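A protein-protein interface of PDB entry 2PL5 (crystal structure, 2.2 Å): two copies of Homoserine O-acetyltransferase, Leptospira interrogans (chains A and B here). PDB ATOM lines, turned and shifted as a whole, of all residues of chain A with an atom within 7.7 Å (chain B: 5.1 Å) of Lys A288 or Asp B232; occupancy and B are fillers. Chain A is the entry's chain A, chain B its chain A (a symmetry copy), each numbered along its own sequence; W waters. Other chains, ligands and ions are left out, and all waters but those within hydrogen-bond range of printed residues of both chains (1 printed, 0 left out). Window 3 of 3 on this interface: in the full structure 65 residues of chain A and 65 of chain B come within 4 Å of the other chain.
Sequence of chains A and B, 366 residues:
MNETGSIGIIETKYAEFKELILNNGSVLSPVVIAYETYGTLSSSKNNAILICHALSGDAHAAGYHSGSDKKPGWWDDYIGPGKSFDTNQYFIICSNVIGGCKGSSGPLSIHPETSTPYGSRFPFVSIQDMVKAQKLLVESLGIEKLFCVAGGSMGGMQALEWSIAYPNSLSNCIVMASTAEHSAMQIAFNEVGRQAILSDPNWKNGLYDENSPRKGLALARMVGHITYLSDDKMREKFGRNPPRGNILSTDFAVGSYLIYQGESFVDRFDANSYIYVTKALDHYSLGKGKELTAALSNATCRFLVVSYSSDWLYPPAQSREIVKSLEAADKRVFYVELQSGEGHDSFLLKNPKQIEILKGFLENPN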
ATOM      1  N   ALA A 180       5.450  -1.237  -2.162  1.00  0.00           N
ATOM      2  CA  ALA A 180       5.041  -2.616  -2.405  1.00  0.00           C
ATOM      3  C   ALA A 180       4.652  -2.835  -3.867  1.00  0.00           C
ATOM      4  O   ALA A 180       4.565  -3.979  -4.336  1.00  0.00           O
ATOM      5  CB  ALA A 180       3.875  -2.978  -1.480  1.00  0.00           C
ATOM      6  N   GLU A 181       4.405  -1.733  -4.579  1.00  0.00           N
ATOM      7  CA  GLU A 181       4.141  -1.757  -6.021  1.00  0.00           C
ATOM      8  C   GLU A 181       4.287  -0.360  -6.620  1.00  0.00           C
ATOM      9  O   GLU A 181       3.929   0.641  -5.981  1.00  0.00           O
ATOM     10  CB  GLU A 181       2.741  -2.296  -6.307  1.00  0.00           C
ATOM     11  CG  GLU A 181       1.620  -1.616  -5.502  1.00  0.00           C
ATOM     12  CD  GLU A 181       0.240  -2.056  -5.929  1.00  0.00           C
ATOM     13  OE1 GLU A 181       0.109  -3.059  -6.652  1.00  0.00           O
ATOM     14  OE2 GLU A 181      -0.728  -1.389  -5.539  1.00  0.00           O
ATOM     15  N   SER A 183       3.512   2.901  -8.788  1.00  0.00           N
ATOM     16  CA  SER A 183       2.344   3.635  -9.284  1.00  0.00           C
ATOM     17  C   SER A 183       2.396   3.722 -10.804  1.00  0.00           C
ATOM     18  O   SER A 183       3.444   3.452 -11.407  1.00  0.00           O
ATOM     19  CB  SER A 183       2.287   5.039  -8.687  1.00  0.00           C
ATOM     20  OG  SER A 183       3.456   5.771  -8.996  1.00  0.00           O
ATOM     21  N   ALA A 184       1.273   4.097 -11.422  1.00  0.00           N
ATOM     22  CA  ALA A 184       1.249   4.412 -12.859  1.00  0.00           C
ATOM     23  C   ALA A 184       2.308   5.447 -13.228  1.00  0.00           C
ATOM     24  O   ALA A 184       2.914   5.365 -14.296  1.00  0.00           O
ATOM     25  CB  ALA A 184      -0.140   4.898 -13.288  1.00  0.00           C
ATOM     26  N   SER A 285       4.528  -6.603  -7.749  1.00  0.00           N
ATOM     27  CA  SER A 285       3.409  -6.109  -6.942  1.00  0.00           C
ATOM     28  C   SER A 285       3.052  -7.030  -5.778  1.00  0.00           C
ATOM     29  O   SER A 285       2.675  -8.184  -5.977  1.00  0.00           O
ATOM     30  CB  SER A 285       2.171  -5.849  -7.809  1.00  0.00           C
ATOM     31  OG  SER A 285       1.086  -5.391  -7.013  1.00  0.00           O
ATOM     32  N   LEU A 286       3.172  -6.505  -4.561  1.00  0.00           N
ATOM     33  CA  LEU A 286       2.604  -7.172  -3.393  1.00  0.00           C
ATOM     34  C   LEU A 286       1.191  -6.660  -3.132  1.00  0.00           C
ATOM     35  O   LEU A 286       0.466  -7.198  -2.294  1.00  0.00           O
ATOM     36  CB  LEU A 286       3.498  -7.007  -2.162  1.00  0.00           C
ATOM     37  CG  LEU A 286       4.900  -7.628  -2.241  1.00  0.00           C
ATOM     38  CD1 LEU A 286       5.626  -7.476  -0.909  1.00  0.00           C
ATOM     39  CD2 LEU A 286       4.845  -9.098  -2.674  1.00  0.00           C
ATOM     40  N   GLY A 287       0.808  -5.615  -3.864  1.00  0.00           N
ATOM     41  CA  GLY A 287      -0.551  -5.082  -3.827  1.00  0.00           C
ATOM     42  C   GLY A 287      -0.701  -3.992  -2.797  1.00  0.00           C
ATOM     43  O   GLY A 287       0.278  -3.357  -2.396  1.00  0.00           O
ATOM     44  N   LYS A 288      -1.941  -3.767  -2.381  1.00  0.00           N
ATOM     45  CA  LYS A 288      -2.240  -2.806  -1.327  1.00  0.00           C
ATOM     46  C   LYS A 288      -3.455  -3.273  -0.535  1.00  0.00           C
ATOM     47  O   LYS A 288      -4.157  -4.200  -0.960  1.00  0.00           O
ATOM     48  CB  LYS A 288      -2.457  -1.403  -1.906  1.00  0.00           C
ATOM     49  CG  LYS A 288      -3.598  -1.305  -2.899  1.00  0.00           C
ATOM     50  CD  LYS A 288      -3.895   0.142  -3.255  1.00  0.00           C
ATOM     51  CE  LYS A 288      -5.203   0.249  -4.015  1.00  0.00           C
ATOM     52  NZ  LYS A 288      -5.160  -0.540  -5.273  1.00  0.00           N
ATOM     53  N   GLY A 289      -3.694  -2.630   0.607  1.00  0.00           N
ATOM     54  CA  GLY A 289      -4.835  -2.952   1.462  1.00  0.00           C
ATOM     55  C   GLY A 289      -4.797  -4.388   1.949  1.00  0.00           C
ATOM     56  O   GLY A 289      -3.758  -4.870   2.414  1.00  0.00           O
ATOM     57  N   LYS A 290      -5.930  -5.071   1.808  1.00  0.00           N
ATOM     58  CA  LYS A 290      -6.094  -6.451   2.269  1.00  0.00           C
ATOM     59  C   LYS A 290      -5.125  -7.426   1.603  1.00  0.00           C
ATOM     60  O   LYS A 290      -4.610  -8.332   2.262  1.00  0.00           O
ATOM     61  CB  LYS A 290      -7.540  -6.917   2.058  1.00  0.00           C
ATOM     62  N   GLU A 291      -4.891  -7.243   0.301  1.00  0.00           N
ATOM     63  CA  GLU A 291      -3.980  -8.105  -0.455  1.00  0.00           C
ATOM     64  C   GLU A 291      -2.533  -7.964   0.009  1.00  0.00           C
ATOM     65  O   GLU A 291      -1.819  -8.960   0.112  1.00  0.00           O
ATOM     66  CB  GLU A 291      -4.104  -7.865  -1.964  1.00  0.00           C
ATOM     67  CG  GLU A 291      -5.249  -8.655  -2.605  1.00  0.00           C
ATOM     68  CD  GLU A 291      -5.428  -8.375  -4.090  1.00  0.00           C
ATOM     69  OE1 GLU A 291      -6.469  -8.789  -4.642  1.00  0.00           O
ATOM     70  OE2 GLU A 291      -4.542  -7.748  -4.709  1.00  0.00           O
ATOM     71  N   LEU A 292      -2.119  -6.734   0.307  1.00  0.00           N
ATOM     72  CA  LEU A 292      -0.783  -6.478   0.837  1.00  0.00           C
ATOM     73  C   LEU A 292      -0.633  -7.016   2.259  1.00  0.00           C
ATOM     74  O   LEU A 292       0.431  -7.513   2.633  1.00  0.00           O
ATOM     75  CB  LEU A 292      -0.450  -4.984   0.800  1.00  0.00           C
ATOM     76  CG  LEU A 292       0.925  -4.566   1.339  1.00  0.00           C
ATOM     77  CD1 LEU A 292       2.053  -5.231   0.560  1.00  0.00           C
ATOM     78  CD2 LEU A 292       1.098  -3.052   1.351  1.00  0.00           C
ATOM     79  N   THR A 293      -1.692  -6.887   3.054  1.00  0.00           N
ATOM     80  CA  THR A 293      -1.706  -7.429   4.405  1.00  0.00           C
ATOM     81  C   THR A 293      -1.467  -8.938   4.353  1.00  0.00           C
ATOM     82  O   THR A 293      -0.575  -9.445   5.028  1.00  0.00           O
ATOM     83  CB  THR A 293      -3.024  -7.092   5.129  1.00  0.00           C
ATOM     84  OG1 THR A 293      -3.110  -5.672   5.300  1.00  0.00           O
ATOM     85  CG2 THR A 293      -3.091  -7.772   6.504  1.00  0.00           C
ATOM     86  N   ALA A 294      -2.248  -9.624   3.518  1.00  0.00           N
ATOM     87  CA  ALA A 294      -2.132 -11.063   3.293  1.00  0.00           C
ATOM     88  C   ALA A 294      -0.735 -11.476   2.811  1.00  0.00           C
ATOM     89  O   ALA A 294      -0.183 -12.472   3.282  1.00  0.00           O
ATOM     90  CB  ALA A 294      -3.198 -11.521   2.304  1.00  0.00           C
ATOM     91  N   ALA A 295      -0.168 -10.706   1.880  1.00  0.00           N
ATOM     92  CA  ALA A 295       1.170 -10.980   1.343  1.00  0.00           C
ATOM     93  C   ALA A 295       2.259 -10.849   2.405  1.00  0.00           C
ATOM     94  O   ALA A 295       3.212 -11.626   2.415  1.00  0.00           O
ATOM     95  CB  ALA A 295       1.473 -10.070   0.154  1.00  0.00           C
ATOM     96  N   GLU A 321       1.304   2.871   3.278  1.00  0.00           N
ATOM     97  CA  GLU A 321       0.546   1.675   2.891  1.00  0.00           C
ATOM     98  C   GLU A 321       1.219   0.379   3.363  1.00  0.00           C
ATOM     99  O   GLU A 321       0.544  -0.594   3.708  1.00  0.00           O
ATOM    100  CB  GLU A 321       0.340   1.635   1.376  1.00  0.00           C
ATOM    101  CG  GLU A 321      -0.727   0.646   0.918  1.00  0.00           C
ATOM    102  CD  GLU A 321      -2.130   1.053   1.335  1.00  0.00           C
ATOM    103  OE1 GLU A 321      -2.398   2.275   1.434  1.00  0.00           O
ATOM    104  OE2 GLU A 321      -2.970   0.153   1.555  1.00  0.00           O
ATOM    105  N   ILE A 322       2.549   0.383   3.370  1.00  0.00           N
ATOM    106  CA  ILE A 322       3.332  -0.746   3.866  1.00  0.00           C
ATOM    107  C   ILE A 322       3.150  -0.877   5.380  1.00  0.00           C
ATOM    108  O   ILE A 322       2.793  -1.950   5.878  1.00  0.00           O
ATOM    109  CB  ILE A 322       4.840  -0.611   3.483  1.00  0.00           C
ATOM    110  CG1 ILE A 322       5.025  -0.743   1.961  1.00  0.00           C
ATOM    111  CG2 ILE A 322       5.697  -1.648   4.229  1.00  0.00           C
ATOM    112  CD1 ILE A 322       6.379  -0.241   1.447  1.00  0.00           C
ATOM    113  N   SER A 325      -0.346  -2.060   6.364  1.00  0.00           N
ATOM    114  CA  SER A 325      -0.506  -3.496   6.154  1.00  0.00           C
ATOM    115  C   SER A 325       0.335  -4.333   7.123  1.00  0.00           C
ATOM    116  O   SER A 325      -0.057  -5.440   7.478  1.00  0.00           O
ATOM    117  CB  SER A 325      -0.220  -3.877   4.703  1.00  0.00           C
ATOM    118  OG  SER A 325      -1.417  -3.871   3.939  1.00  0.00           O
ATOM    119  N   SER B 230      -4.884   4.791 -15.389  1.00  0.00           N
ATOM    120  CA  SER B 230      -4.945   5.035 -13.945  1.00  0.00           C
ATOM    121  C   SER B 230      -4.001   4.076 -13.218  1.00  0.00           C
ATOM    122  O   SER B 230      -3.467   3.154 -13.837  1.00  0.00           O
ATOM    123  CB  SER B 230      -6.379   4.872 -13.425  1.00  0.00           C
ATOM    124  OG  SER B 230      -6.801   3.520 -13.485  1.00  0.00           O
ATOM    125  N   ASP B 231      -3.789   4.296 -11.921  1.00  0.00           N
ATOM    126  CA  ASP B 231      -2.968   3.385 -11.109  1.00  0.00           C
ATOM    127  C   ASP B 231      -3.439   1.933 -11.202  1.00  0.00           C
ATOM    128  O   ASP B 231      -2.617   1.026 -11.315  1.00  0.00           O
ATOM    129  CB  ASP B 231      -2.937   3.818  -9.638  1.00  0.00           C
ATOM    130  CG  ASP B 231      -2.043   5.018  -9.393  1.00  0.00           C
ATOM    131  OD1 ASP B 231      -1.043   5.202 -10.114  1.00  0.00           O
ATOM    132  OD2 ASP B 231      -2.338   5.787  -8.458  1.00  0.00           O
ATOM    133  N   ASP B 232      -4.759   1.729 -11.159  1.00  0.00           N
ATOM    134  CA  ASP B 232      -5.366   0.393 -11.208  1.00  0.00           C
ATOM    135  C   ASP B 232      -5.251  -0.265 -12.579  1.00  0.00           C
ATOM    136  O   ASP B 232      -4.961  -1.458 -12.673  1.00  0.00           O
ATOM    137  CB  ASP B 232      -6.844   0.439 -10.789  1.00  0.00           C
ATOM    138  CG  ASP B 232      -7.032   0.622  -9.295  1.00  0.00           C
ATOM    139  OD1 ASP B 232      -8.195   0.708  -8.858  1.00  0.00           O
ATOM    140  OD2 ASP B 232      -6.032   0.685  -8.552  1.00  0.00           O
ATOM    141  N   LYS B 233      -5.486   0.508 -13.639  1.00  0.00           N
ATOM    142  CA  LYS B 233      -5.435  -0.038 -14.998  1.00  0.00           C
ATOM    143  C   LYS B 233      -4.010  -0.291 -15.494  1.00  0.00           C
ATOM    144  O   LYS B 233      -3.787  -1.151 -16.358  1.00  0.00           O
ATOM    145  CB  LYS B 233      -6.218   0.844 -15.979  1.00  0.00           C
ATOM    146  CG  LYS B 233      -7.733   0.799 -15.768  1.00  0.00           C
ATOM    147  CD  LYS B 233      -8.319  -0.586 -16.051  1.00  0.00           C
ATOM    148  CE  LYS B 233      -9.713  -0.725 -15.461  1.00  0.00           C
ATOM    149  NZ  LYS B 233     -10.234  -2.126 -15.572  1.00  0.00           N
ATOM    150  N   MET B 234      -3.059   0.461 -14.945  1.00  0.00           N
ATOM    151  CA  MET B 234      -1.638   0.265 -15.234  1.00  0.00           C
ATOM    152  C   MET B 234      -1.116  -0.990 -14.525  1.00  0.00           C
ATOM    153  O   MET B 234      -0.338  -1.754 -15.093  1.00  0.00           O
ATOM    154  CB  MET B 234      -0.834   1.496 -14.804  1.00  0.00           C
ATOM    155  CG  MET B 234       0.612   1.482 -15.256  1.00  0.00           C
ATOM    156  SD  MET B 234       0.813   1.794 -17.022  1.00  0.00           S
ATOM    157  CE  MET B 234       0.863   3.584 -17.008  1.00  0.00           C
ATOM    158  N   ARG B 235      -1.552  -1.188 -13.283  1.00  0.00           N
ATOM    159  CA  ARG B 235      -1.207  -2.381 -12.511  1.00  0.00           C
ATOM    160  C   ARG B 235      -1.833  -3.636 -13.126  1.00  0.00           C
ATOM    161  O   ARG B 235      -1.215  -4.705 -13.143  1.00  0.00           O
ATOM    162  CB  ARG B 235      -1.609  -2.209 -11.044  1.00  0.00           C
ATOM    163  CG  ARG B 235      -1.396  -3.437 -10.143  1.00  0.00           C
ATOM    164  CD  ARG B 235       0.014  -3.982 -10.251  1.00  0.00           C
ATOM    165  NE  ARG B 235       1.032  -2.966  -9.988  1.00  0.00           N
ATOM    166  CZ  ARG B 235       2.271  -3.009 -10.470  1.00  0.00           C
ATOM    167  NH1 ARG B 235       2.650  -4.014 -11.256  1.00  0.00           N
ATOM    168  NH2 ARG B 235       3.128  -2.047 -10.178  1.00  0.00           N
ATOM    169  N   GLU B 236      -3.047  -3.489 -13.652  1.00  0.00           N
ATOM    170  CA  GLU B 236      -3.718  -4.566 -14.355  1.00  0.00           C
ATOM    171  C   GLU B 236      -2.914  -4.991 -15.580  1.00  0.00           C
ATOM    172  O   GLU B 236      -2.705  -6.187 -15.804  1.00  0.00           O
ATOM    173  CB  GLU B 236      -5.130  -4.134 -14.750  1.00  0.00           C
ATOM    174  CG  GLU B 236      -6.082  -5.282 -15.029  1.00  0.00           C
ATOM    175  CD  GLU B 236      -7.493  -4.803 -15.311  1.00  0.00           C
ATOM    176  OE1 GLU B 236      -8.057  -4.054 -14.475  1.00  0.00           O
ATOM    177  OE2 GLU B 236      -8.034  -5.175 -16.373  1.00  0.00           O
HETATM  178  O   HOH W   1       0.446  -0.306  -8.616  1.00  0.00           O
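Asp B232 touches just one residue of chain A: Lys A288 (3.6 Å). Of the printed residues of chain B, Ser A183 touches Asp B231. Of the printed residues of chain A, Arg B235 touches Glu A181 (3.5 Å) and Ser A285 (3.7 Å). Printed residues of chain A within 4 Å of Asp B231: Ser A183 and Ala A184. Of the printed residues of chain B, Ser A285 touches Arg B235. The nearest printed residue of chain A that does not touch Met B234 is Ser A183 (5.2 Å).
The side-chain hydroxyl (OG) of Ser A285 lies within hydrogen-bond range of the side-chain carboxylate (OE1) of Glu A181 (2.6 Å). The side-chain hydroxyl of Ser A285 lies within hydrogen-bond range of the backbone NH of Gly A287 (3.2 Å). N of Lys B233 is in hydrogen-bond range of OG of Ser B230 (3.3 Å).
Hydrophobic or aromatic side chains of chain B within 4 Å of the printed part of chain A: Met B234. Of the 18 printed residues of chain A, 5 touch a printed residue of chain B. Along chain A the printed residues that touch a printed residue of chain B span positions 181 to 288. Among the printed residues, 7 pairs touch across the chains.
No position is printed for both chains. Of the 7 pairs that touch across the chains among the printed residues, none has its exchanged pair printed and touching as well.
Among the printed residues, merely in contact across the chains: Ser A183 with Asp B231 (3.6 Å), Ser A285 with Arg B235 (3.7 Å), Ala A184 with Met B234 (3.8 Å) and Ala A184 with Ser B230 (3.8 Å).
Water W1 lies within hydrogen-bond range of NE of Arg B235 and OE1 of Glu A181.
The side-chain carboxylate of Glu A181 is in salt-bridge range of the guanidinium group of Arg B235 (3.5 Å). The backbone NH (N) of Ala A184 lies within hydrogen-bond range of the side-chain carboxylate (OD1) of Asp B231, 2.9 Å away. NZ of Lys A288 lies within salt-bridge range of OD2 of Asp B232.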
